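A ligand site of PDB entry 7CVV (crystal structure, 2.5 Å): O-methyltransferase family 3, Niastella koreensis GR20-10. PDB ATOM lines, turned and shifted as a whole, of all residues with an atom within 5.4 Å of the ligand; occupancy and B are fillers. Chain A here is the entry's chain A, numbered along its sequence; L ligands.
Merely in contact with the ligand: Ile 39, Ser 40, Thr 66, Asp 91, Lys 117, Phe 137 and Ala 140.
Within 4 Å of the ligand: Ile 39, Ser 40, Val 41, Gly 65, Thr 66, Leu 67, Tyr 70, Ser 71, Glu 89, Tyr 90, Asp 91, His 94, Lys 117, Ala 118, Phe 137, Asp 139, Ala 140, Asp 141 and Tyr 148.
The nearest printed residue that does not touch the ligand is Gly 116 (4.02 Å).
OE2 of Glu 89 sits at hydrogen-bond distance from O5 of the ligand, 2.5 Å away.
A nitrogen (N1) of the ligand is in salt-bridge range of the side-chain carboxylate (OD2) of Asp 139, 2.6 Å away.
O2 of the ligand lies within hydrogen-bond range of N of Val 41 (2.8 Å).
The side-chain carboxylate (OD1) of Asp 141 is in hydrogen-bond range of a nitrogen (N4) of the ligand (2.9 Å).
A ring nitrogen (ND1) of His 94 sits at hydrogen-bond distance from an oxygen (O4) of the ligand (2.9 Å).
An oxygen (O1) of the ligand sits at hydrogen-bond distance from the backbone NH of Ser 71 (3.2 Å).
A nitrogen (N1) of the ligand is in hydrogen-bond range of the side-chain hydroxyl (OG) of Ser 71 (3.1 Å).
N of Tyr 90 lies within hydrogen-bond range of N6 of the ligand, at 3.2 Å.
A nitrogen (N4) of the ligand lies within hydrogen-bond range of the side-chain hydroxyl (OH) of Tyr 148 (3.2 Å).
A nitrogen (N5) of the ligand sits at hydrogen-bond distance from the backbone NH (N) of Ala 118, 3.3 Å away.
A nitrogen (N1) of the ligand sits at hydrogen-bond distance from the backbone carbonyl oxygen (O) of Gly 65, at 3.3 Å.
N of Leu 67 lies close to O4 of the ligand (3.4 Å).
The backbone NH (N) of Tyr 70 sits close to an oxygen (O1) of the ligand (3.5 Å).
N of Leu 67 is in hydrogen-bond range of OE1 of Glu 89 (3.2 Å).
The side-chain carboxylate of Glu 89 is in hydrogen-bond range of the backbone NH of Thr 66 (3.3 Å).
OE2 of Glu 89 sits at hydrogen-bond distance from N of Asp 91 (2.8 Å).
The backbone NH of Gly 116 lies within hydrogen-bond range of the backbone carbonyl oxygen of Glu 89 (3.0 Å).
The side-chain carboxylate of Asp 141 lies within hydrogen-bond range of the side-chain hydroxyl of Tyr 148, 2.5 Å away.
The backbone NH (N) of Gly 65 lies within hydrogen-bond range of the backbone carbonyl oxygen (O) of Leu 88, at 2.7 Å.
OG1 of Thr 66 lies within hydrogen-bond range of O of Leu 88, at 3.1 Å.
The backbone NH of Leu 64 sits at hydrogen-bond distance from the backbone carbonyl oxygen of Phe 137.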
ATOM      1  N   ILE A  39     -22.530  20.238  -0.119  1.00  0.00           N
ATOM      2  CA  ILE A  39     -22.969  19.185  -1.088  1.00  0.00           C
ATOM      3  C   ILE A  39     -21.976  18.013  -1.027  1.00  0.00           C
ATOM      4  O   ILE A  39     -21.831  17.293  -2.055  1.00  0.00           O
ATOM      5  CB  ILE A  39     -23.135  19.757  -2.509  1.00  0.00           C
ATOM      6  CG1 ILE A  39     -21.828  20.355  -3.048  1.00  0.00           C
ATOM      7  CG2 ILE A  39     -24.285  20.758  -2.523  1.00  0.00           C
ATOM      8  CD1 ILE A  39     -21.838  20.632  -4.535  1.00  0.00           C
ATOM      9  N   SER A  40     -21.359  17.799   0.131  1.00  0.00           N
ATOM     10  CA  SER A  40     -20.418  16.682   0.374  1.00  0.00           C
ATOM     11  C   SER A  40     -21.200  15.382   0.637  1.00  0.00           C
ATOM     12  O   SER A  40     -22.413  15.464   0.948  1.00  0.00           O
ATOM     13  CB  SER A  40     -19.435  17.015   1.470  1.00  0.00           C
ATOM     14  OG  SER A  40     -19.950  16.653   2.751  1.00  0.00           O
ATOM     15  N   VAL A  41     -20.533  14.233   0.527  1.00  0.00           N
ATOM     16  CA  VAL A  41     -21.079  12.947   1.027  1.00  0.00           C
ATOM     17  C   VAL A  41     -21.320  13.086   2.528  1.00  0.00           C
ATOM     18  O   VAL A  41     -20.731  13.965   3.137  1.00  0.00           O
ATOM     19  CB  VAL A  41     -20.169  11.737   0.715  1.00  0.00           C
ATOM     20  CG1 VAL A  41     -19.946  11.611  -0.777  1.00  0.00           C
ATOM     21  CG2 VAL A  41     -18.848  11.781   1.486  1.00  0.00           C
ATOM     22  N   GLU A  63     -10.694  10.386  -8.360  1.00  0.00           N
ATOM     23  CA  GLU A  63     -11.858  11.130  -7.810  1.00  0.00           C
ATOM     24  C   GLU A  63     -12.120  12.322  -8.735  1.00  0.00           C
ATOM     25  O   GLU A  63     -11.196  13.128  -8.911  1.00  0.00           O
ATOM     26  CB  GLU A  63     -11.569  11.591  -6.388  1.00  0.00           C
ATOM     27  CG  GLU A  63     -12.752  12.291  -5.742  1.00  0.00           C
ATOM     28  CD  GLU A  63     -12.562  12.814  -4.327  1.00  0.00           C
ATOM     29  OE1 GLU A  63     -13.519  12.670  -3.529  1.00  0.00           O
ATOM     30  OE2 GLU A  63     -11.483  13.380  -4.005  1.00  0.00           O
ATOM     31  N   LEU A  64     -13.319  12.413  -9.306  1.00  0.00           N
ATOM     32  CA  LEU A  64     -13.781  13.643  -9.996  1.00  0.00           C
ATOM     33  C   LEU A  64     -14.630  14.447  -9.012  1.00  0.00           C
ATOM     34  O   LEU A  64     -15.693  13.998  -8.688  1.00  0.00           O
ATOM     35  CB  LEU A  64     -14.615  13.294 -11.229  1.00  0.00           C
ATOM     36  CG  LEU A  64     -13.977  12.348 -12.244  1.00  0.00           C
ATOM     37  CD1 LEU A  64     -14.411  12.718 -13.652  1.00  0.00           C
ATOM     38  CD2 LEU A  64     -12.470  12.356 -12.151  1.00  0.00           C
ATOM     39  N   GLY A  65     -14.190  15.627  -8.611  1.00  0.00           N
ATOM     40  CA  GLY A  65     -14.975  16.509  -7.742  1.00  0.00           C
ATOM     41  C   GLY A  65     -14.494  16.392  -6.318  1.00  0.00           C
ATOM     42  O   GLY A  65     -14.919  15.436  -5.627  1.00  0.00           O
ATOM     43  N   THR A  66     -13.594  17.300  -5.933  1.00  0.00           N
ATOM     44  CA  THR A  66     -12.904  17.354  -4.619  1.00  0.00           C
ATOM     45  C   THR A  66     -13.782  18.089  -3.604  1.00  0.00           C
ATOM     46  O   THR A  66     -13.979  17.536  -2.508  1.00  0.00           O
ATOM     47  CB  THR A  66     -11.517  17.996  -4.810  1.00  0.00           C
ATOM     48  OG1 THR A  66     -10.928  17.406  -5.983  1.00  0.00           O
ATOM     49  CG2 THR A  66     -10.601  17.782  -3.626  1.00  0.00           C
ATOM     50  N   LEU A  67     -14.301  19.273  -3.964  1.00  0.00           N
ATOM     51  CA  LEU A  67     -14.928  20.267  -3.056  1.00  0.00           C
ATOM     52  C   LEU A  67     -13.944  20.584  -1.922  1.00  0.00           C
ATOM     53  O   LEU A  67     -12.815  20.956  -2.250  1.00  0.00           O
ATOM     54  CB  LEU A  67     -16.271  19.707  -2.568  1.00  0.00           C
ATOM     55  CG  LEU A  67     -17.243  20.757  -2.003  1.00  0.00           C
ATOM     56  CD1 LEU A  67     -17.843  21.615  -3.114  1.00  0.00           C
ATOM     57  CD2 LEU A  67     -18.336  20.097  -1.194  1.00  0.00           C
ATOM     58  N   ALA A  68     -14.301  20.415  -0.653  1.00  0.00           N
ATOM     59  CA  ALA A  68     -13.392  20.709   0.481  1.00  0.00           C
ATOM     60  C   ALA A  68     -12.546  19.472   0.818  1.00  0.00           C
ATOM     61  O   ALA A  68     -11.753  19.551   1.781  1.00  0.00           O
ATOM     62  CB  ALA A  68     -14.170  21.167   1.692  1.00  0.00           C
ATOM     63  N   GLY A  69     -12.708  18.391   0.051  1.00  0.00           N
ATOM     64  CA  GLY A  69     -11.985  17.120   0.227  1.00  0.00           C
ATOM     65  C   GLY A  69     -12.505  16.258   1.363  1.00  0.00           C
ATOM     66  O   GLY A  69     -11.726  15.473   1.897  1.00  0.00           O
ATOM     67  N   TYR A  70     -13.785  16.348   1.714  1.00  0.00           N
ATOM     68  CA  TYR A  70     -14.421  15.469   2.735  1.00  0.00           C
ATOM     69  C   TYR A  70     -14.321  13.997   2.289  1.00  0.00           C
ATOM     70  O   TYR A  70     -13.729  13.170   3.011  1.00  0.00           O
ATOM     71  CB  TYR A  70     -15.840  15.964   3.011  1.00  0.00           C
ATOM     72  CG  TYR A  70     -16.551  15.210   4.094  1.00  0.00           C
ATOM     73  CD1 TYR A  70     -17.282  14.071   3.812  1.00  0.00           C
ATOM     74  CD2 TYR A  70     -16.509  15.641   5.407  1.00  0.00           C
ATOM     75  CE1 TYR A  70     -17.933  13.355   4.796  1.00  0.00           C
ATOM     76  CE2 TYR A  70     -17.160  14.956   6.411  1.00  0.00           C
ATOM     77  CZ  TYR A  70     -17.860  13.798   6.109  1.00  0.00           C
ATOM     78  OH  TYR A  70     -18.488  13.120   7.118  1.00  0.00           O
ATOM     79  N   SER A  71     -14.816  13.682   1.084  1.00  0.00           N
ATOM     80  CA  SER A  71     -14.837  12.305   0.514  1.00  0.00           C
ATOM     81  C   SER A  71     -13.408  11.812   0.323  1.00  0.00           C
ATOM     82  O   SER A  71     -13.167  10.622   0.515  1.00  0.00           O
ATOM     83  CB  SER A  71     -15.567  12.262  -0.786  1.00  0.00           C
ATOM     84  OG  SER A  71     -14.989  13.188  -1.686  1.00  0.00           O
ATOM     85  N   THR A  72     -12.538  12.733  -0.060  1.00  0.00           N
ATOM     86  CA  THR A  72     -11.086  12.511  -0.293  1.00  0.00           C
ATOM     87  C   THR A  72     -10.445  11.950   0.980  1.00  0.00           C
ATOM     88  O   THR A  72      -9.790  10.897   0.879  1.00  0.00           O
ATOM     89  CB  THR A  72     -10.445  13.819  -0.806  1.00  0.00           C
ATOM     90  OG1 THR A  72     -11.314  14.381  -1.793  1.00  0.00           O
ATOM     91  CG2 THR A  72      -9.068  13.585  -1.379  1.00  0.00           C
ATOM     92  N   LEU A  88      -9.694  15.458  -8.979  1.00  0.00           N
ATOM     93  CA  LEU A  88      -9.817  16.566  -9.960  1.00  0.00           C
ATOM     94  C   LEU A  88     -10.869  17.581  -9.487  1.00  0.00           C
ATOM     95  O   LEU A  88     -11.943  17.147  -8.951  1.00  0.00           O
ATOM     96  CB  LEU A  88     -10.155  15.996 -11.344  1.00  0.00           C
ATOM     97  CG  LEU A  88      -9.376  14.738 -11.734  1.00  0.00           C
ATOM     98  CD1 LEU A  88      -9.587  14.344 -13.195  1.00  0.00           C
ATOM     99  CD2 LEU A  88      -7.886  14.911 -11.441  1.00  0.00           C
ATOM    100  N   GLU A  89     -10.566  18.878  -9.659  1.00  0.00           N
ATOM    101  CA  GLU A  89     -11.396  20.025  -9.175  1.00  0.00           C
ATOM    102  C   GLU A  89     -11.282  21.214 -10.139  1.00  0.00           C
ATOM    103  O   GLU A  89     -10.181  21.748 -10.296  1.00  0.00           O
ATOM    104  CB  GLU A  89     -10.958  20.424  -7.754  1.00  0.00           C
ATOM    105  CG  GLU A  89     -11.741  21.577  -7.183  1.00  0.00           C
ATOM    106  CD  GLU A  89     -13.262  21.438  -7.343  1.00  0.00           C
ATOM    107  OE1 GLU A  89     -13.818  20.408  -6.895  1.00  0.00           O
ATOM    108  OE2 GLU A  89     -13.874  22.361  -7.925  1.00  0.00           O
ATOM    109  N   TYR A  90     -12.398  21.628 -10.738  1.00  0.00           N
ATOM    110  CA  TYR A  90     -12.454  22.772 -11.689  1.00  0.00           C
ATOM    111  C   TYR A  90     -12.138  24.077 -10.947  1.00  0.00           C
ATOM    112  O   TYR A  90     -11.555  24.994 -11.519  1.00  0.00           O
ATOM    113  CB  TYR A  90     -13.824  22.803 -12.361  1.00  0.00           C
ATOM    114  CG  TYR A  90     -14.114  24.023 -13.184  1.00  0.00           C
ATOM    115  CD1 TYR A  90     -13.623  24.151 -14.482  1.00  0.00           C
ATOM    116  CD2 TYR A  90     -14.946  25.022 -12.709  1.00  0.00           C
ATOM    117  CE1 TYR A  90     -13.920  25.256 -15.271  1.00  0.00           C
ATOM    118  CE2 TYR A  90     -15.261  26.130 -13.474  1.00  0.00           C
ATOM    119  CZ  TYR A  90     -14.742  26.244 -14.761  1.00  0.00           C
ATOM    120  OH  TYR A  90     -15.049  27.352 -15.506  1.00  0.00           O
ATOM    121  N   ASP A  91     -12.530  24.152  -9.688  1.00  0.00           N
ATOM    122  CA  ASP A  91     -12.635  25.420  -8.927  1.00  0.00           C
ATOM    123  C   ASP A  91     -11.371  25.607  -8.082  1.00  0.00           C
ATOM    124  O   ASP A  91     -11.102  24.838  -7.166  1.00  0.00           O
ATOM    125  CB  ASP A  91     -13.948  25.453  -8.148  1.00  0.00           C
ATOM    126  CG  ASP A  91     -14.256  26.847  -7.649  1.00  0.00           C
ATOM    127  OD1 ASP A  91     -13.322  27.502  -7.121  1.00  0.00           O
ATOM    128  OD2 ASP A  91     -15.390  27.279  -7.840  1.00  0.00           O
ATOM    129  N   HIS A  94     -11.905  25.914  -4.400  1.00  0.00           N
ATOM    130  CA  HIS A  94     -12.254  24.573  -3.869  1.00  0.00           C
ATOM    131  C   HIS A  94     -10.948  23.798  -3.663  1.00  0.00           C
ATOM    132  O   HIS A  94     -10.706  23.362  -2.533  1.00  0.00           O
ATOM    133  CB  HIS A  94     -13.284  23.884  -4.758  1.00  0.00           C
ATOM    134  CG  HIS A  94     -14.623  24.555  -4.789  1.00  0.00           C
ATOM    135  ND1 HIS A  94     -15.745  23.974  -5.357  1.00  0.00           N
ATOM    136  CD2 HIS A  94     -15.021  25.781  -4.352  1.00  0.00           C
ATOM    137  CE1 HIS A  94     -16.773  24.799  -5.259  1.00  0.00           C
ATOM    138  NE2 HIS A  94     -16.347  25.915  -4.637  1.00  0.00           N
ATOM    139  N   GLY A 116      -8.512  22.100 -12.804  1.00  0.00           N
ATOM    140  CA  GLY A 116      -8.865  22.124 -14.236  1.00  0.00           C
ATOM    141  C   GLY A 116     -10.114  21.299 -14.507  1.00  0.00           C
ATOM    142  O   GLY A 116     -10.577  20.620 -13.569  1.00  0.00           O
ATOM    143  N   LYS A 117     -10.660  21.372 -15.731  1.00  0.00           N
ATOM    144  CA  LYS A 117     -11.835  20.561 -16.139  1.00  0.00           C
ATOM    145  C   LYS A 117     -11.400  19.099 -16.158  1.00  0.00           C
ATOM    146  O   LYS A 117     -10.305  18.809 -16.662  1.00  0.00           O
ATOM    147  CB  LYS A 117     -12.402  20.967 -17.496  1.00  0.00           C
ATOM    148  CG  LYS A 117     -13.249  22.224 -17.472  1.00  0.00           C
ATOM    149  CD  LYS A 117     -13.213  23.034 -18.757  1.00  0.00           C
ATOM    150  CE  LYS A 117     -14.224  22.564 -19.786  1.00  0.00           C
ATOM    151  NZ  LYS A 117     -14.165  23.393 -21.017  1.00  0.00           N
ATOM    152  N   ALA A 118     -12.226  18.211 -15.621  1.00  0.00           N
ATOM    153  CA  ALA A 118     -12.070  16.735 -15.674  1.00  0.00           C
ATOM    154  C   ALA A 118     -11.847  16.304 -17.128  1.00  0.00           C
ATOM    155  O   ALA A 118     -10.895  15.583 -17.349  1.00  0.00           O
ATOM    156  CB  ALA A 118     -13.273  16.057 -15.057  1.00  0.00           C
ATOM    157  N   PHE A 137     -14.095   7.365  -8.312  1.00  0.00           N
ATOM    158  CA  PHE A 137     -15.276   8.035  -7.742  1.00  0.00           C
ATOM    159  C   PHE A 137     -15.604   9.235  -8.626  1.00  0.00           C
ATOM    160  O   PHE A 137     -14.790  10.167  -8.669  1.00  0.00           O
ATOM    161  CB  PHE A 137     -15.005   8.459  -6.303  1.00  0.00           C
ATOM    162  CG  PHE A 137     -16.194   9.024  -5.594  1.00  0.00           C
ATOM    163  CD1 PHE A 137     -17.451   8.434  -5.736  1.00  0.00           C
ATOM    164  CD2 PHE A 137     -16.085  10.151  -4.782  1.00  0.00           C
ATOM    165  CE1 PHE A 137     -18.558   8.961  -5.081  1.00  0.00           C
ATOM    166  CE2 PHE A 137     -17.201  10.678  -4.147  1.00  0.00           C
ATOM    167  CZ  PHE A 137     -18.430  10.084  -4.292  1.00  0.00           C
ATOM    168  N   ASP A 139     -18.184  12.336  -9.141  1.00  0.00           N
ATOM    169  CA  ASP A 139     -19.037  13.201  -8.276  1.00  0.00           C
ATOM    170  C   ASP A 139     -18.850  14.672  -8.699  1.00  0.00           C
ATOM    171  O   ASP A 139     -18.691  15.554  -7.815  1.00  0.00           O
ATOM    172  CB  ASP A 139     -18.717  12.979  -6.796  1.00  0.00           C
ATOM    173  CG  ASP A 139     -19.801  13.452  -5.843  1.00  0.00           C
ATOM    174  OD1 ASP A 139     -21.009  13.336  -6.205  1.00  0.00           O
ATOM    175  OD2 ASP A 139     -19.426  13.937  -4.726  1.00  0.00           O
ATOM    176  N   ALA A 140     -18.854  14.957 -10.007  1.00  0.00           N
ATOM    177  CA  ALA A 140     -18.684  16.314 -10.568  1.00  0.00           C
ATOM    178  C   ALA A 140     -20.014  16.770 -11.201  1.00  0.00           C
ATOM    179  O   ALA A 140     -21.081  16.242 -10.804  1.00  0.00           O
ATOM    180  CB  ALA A 140     -17.547  16.301 -11.541  1.00  0.00           C
ATOM    181  N   ASP A 141     -19.961  17.728 -12.144  1.00  0.00           N
ATOM    182  CA  ASP A 141     -21.118  18.112 -13.006  1.00  0.00           C
ATOM    183  C   ASP A 141     -21.678  16.820 -13.626  1.00  0.00           C
ATOM    184  O   ASP A 141     -20.893  15.887 -13.891  1.00  0.00           O
ATOM    185  CB  ASP A 141     -20.737  19.192 -14.017  1.00  0.00           C
ATOM    186  CG  ASP A 141     -19.541  18.902 -14.917  1.00  0.00           C
ATOM    187  OD1 ASP A 141     -18.596  18.190 -14.481  1.00  0.00           O
ATOM    188  OD2 ASP A 141     -19.540  19.429 -16.057  1.00  0.00           O
ATOM    189  N   TYR A 148     -17.294  10.939 -18.766  1.00  0.00           N
ATOM    190  CA  TYR A 148     -16.358  10.703 -17.631  1.00  0.00           C
ATOM    191  C   TYR A 148     -16.169   9.200 -17.474  1.00  0.00           C
ATOM    192  O   TYR A 148     -15.047   8.766 -17.194  1.00  0.00           O
ATOM    193  CB  TYR A 148     -16.893  11.327 -16.339  1.00  0.00           C
ATOM    194  CG  TYR A 148     -16.935  12.833 -16.273  1.00  0.00           C
ATOM    195  CD1 TYR A 148     -15.982  13.622 -16.891  1.00  0.00           C
ATOM    196  CD2 TYR A 148     -17.917  13.469 -15.539  1.00  0.00           C
ATOM    197  CE1 TYR A 148     -16.006  15.001 -16.812  1.00  0.00           C
ATOM    198  CE2 TYR A 148     -17.961  14.848 -15.446  1.00  0.00           C
ATOM    199  CZ  TYR A 148     -17.000  15.612 -16.088  1.00  0.00           C
ATOM    200  OH  TYR A 148     -17.047  16.965 -15.985  1.00  0.00           O
HETATM  201  N1  LIG L   1     -17.217  14.427  -3.427  1.00  0.00           N
HETATM  202  C1  LIG L   1     -16.977  15.649  -2.608  1.00  0.00           C
HETATM  203  C2  LIG L   1     -17.255  15.331  -1.134  1.00  0.00           C
HETATM  204  O1  LIG L   1     -16.582  15.920  -0.267  1.00  0.00           O
HETATM  205  O2  LIG L   1     -18.129  14.479  -0.884  1.00  0.00           O
HETATM  206  C3  LIG L   1     -17.897  16.781  -3.077  1.00  0.00           C
HETATM  207  C4  LIG L   1     -17.774  17.180  -4.567  1.00  0.00           C
HETATM  208  S1  LIG L   1     -19.142  18.325  -4.935  1.00  0.00           S
HETATM  209  C5  LIG L   1     -20.478  17.149  -5.113  1.00  0.00           C
HETATM  210  C6  LIG L   1     -18.897  18.832  -6.659  1.00  0.00           C
HETATM  211  C7  LIG L   1     -17.544  19.400  -6.989  1.00  0.00           C
HETATM  212  O3  LIG L   1     -17.287  19.164  -8.403  1.00  0.00           O
HETATM  213  C8  LIG L   1     -17.376  20.904  -6.773  1.00  0.00           C
HETATM  214  O4  LIG L   1     -16.193  21.146  -6.022  1.00  0.00           O
HETATM  215  C9  LIG L   1     -17.220  21.465  -8.189  1.00  0.00           C
HETATM  216  O5  LIG L   1     -16.323  22.545  -8.280  1.00  0.00           O
HETATM  217  C10 LIG L   1     -16.602  20.274  -8.903  1.00  0.00           C
HETATM  218  N2  LIG L   1     -16.763  20.291 -10.353  1.00  0.00           N
HETATM  219  C11 LIG L   1     -17.893  20.675 -11.035  1.00  0.00           C
HETATM  220  N3  LIG L   1     -17.763  20.560 -12.333  1.00  0.00           N
HETATM  221  C12 LIG L   1     -16.493  20.056 -12.516  1.00  0.00           C
HETATM  222  C13 LIG L   1     -15.772  19.710 -13.673  1.00  0.00           C
HETATM  223  N4  LIG L   1     -16.278  19.855 -14.898  1.00  0.00           N
HETATM  224  N5  LIG L   1     -14.532  19.196 -13.522  1.00  0.00           N
HETATM  225  C14 LIG L   1     -14.051  19.063 -12.276  1.00  0.00           C
HETATM  226  N6  LIG L   1     -14.624  19.387 -11.113  1.00  0.00           N
HETATM  227  C15 LIG L   1     -15.857  19.871 -11.297  1.00  0.00           C
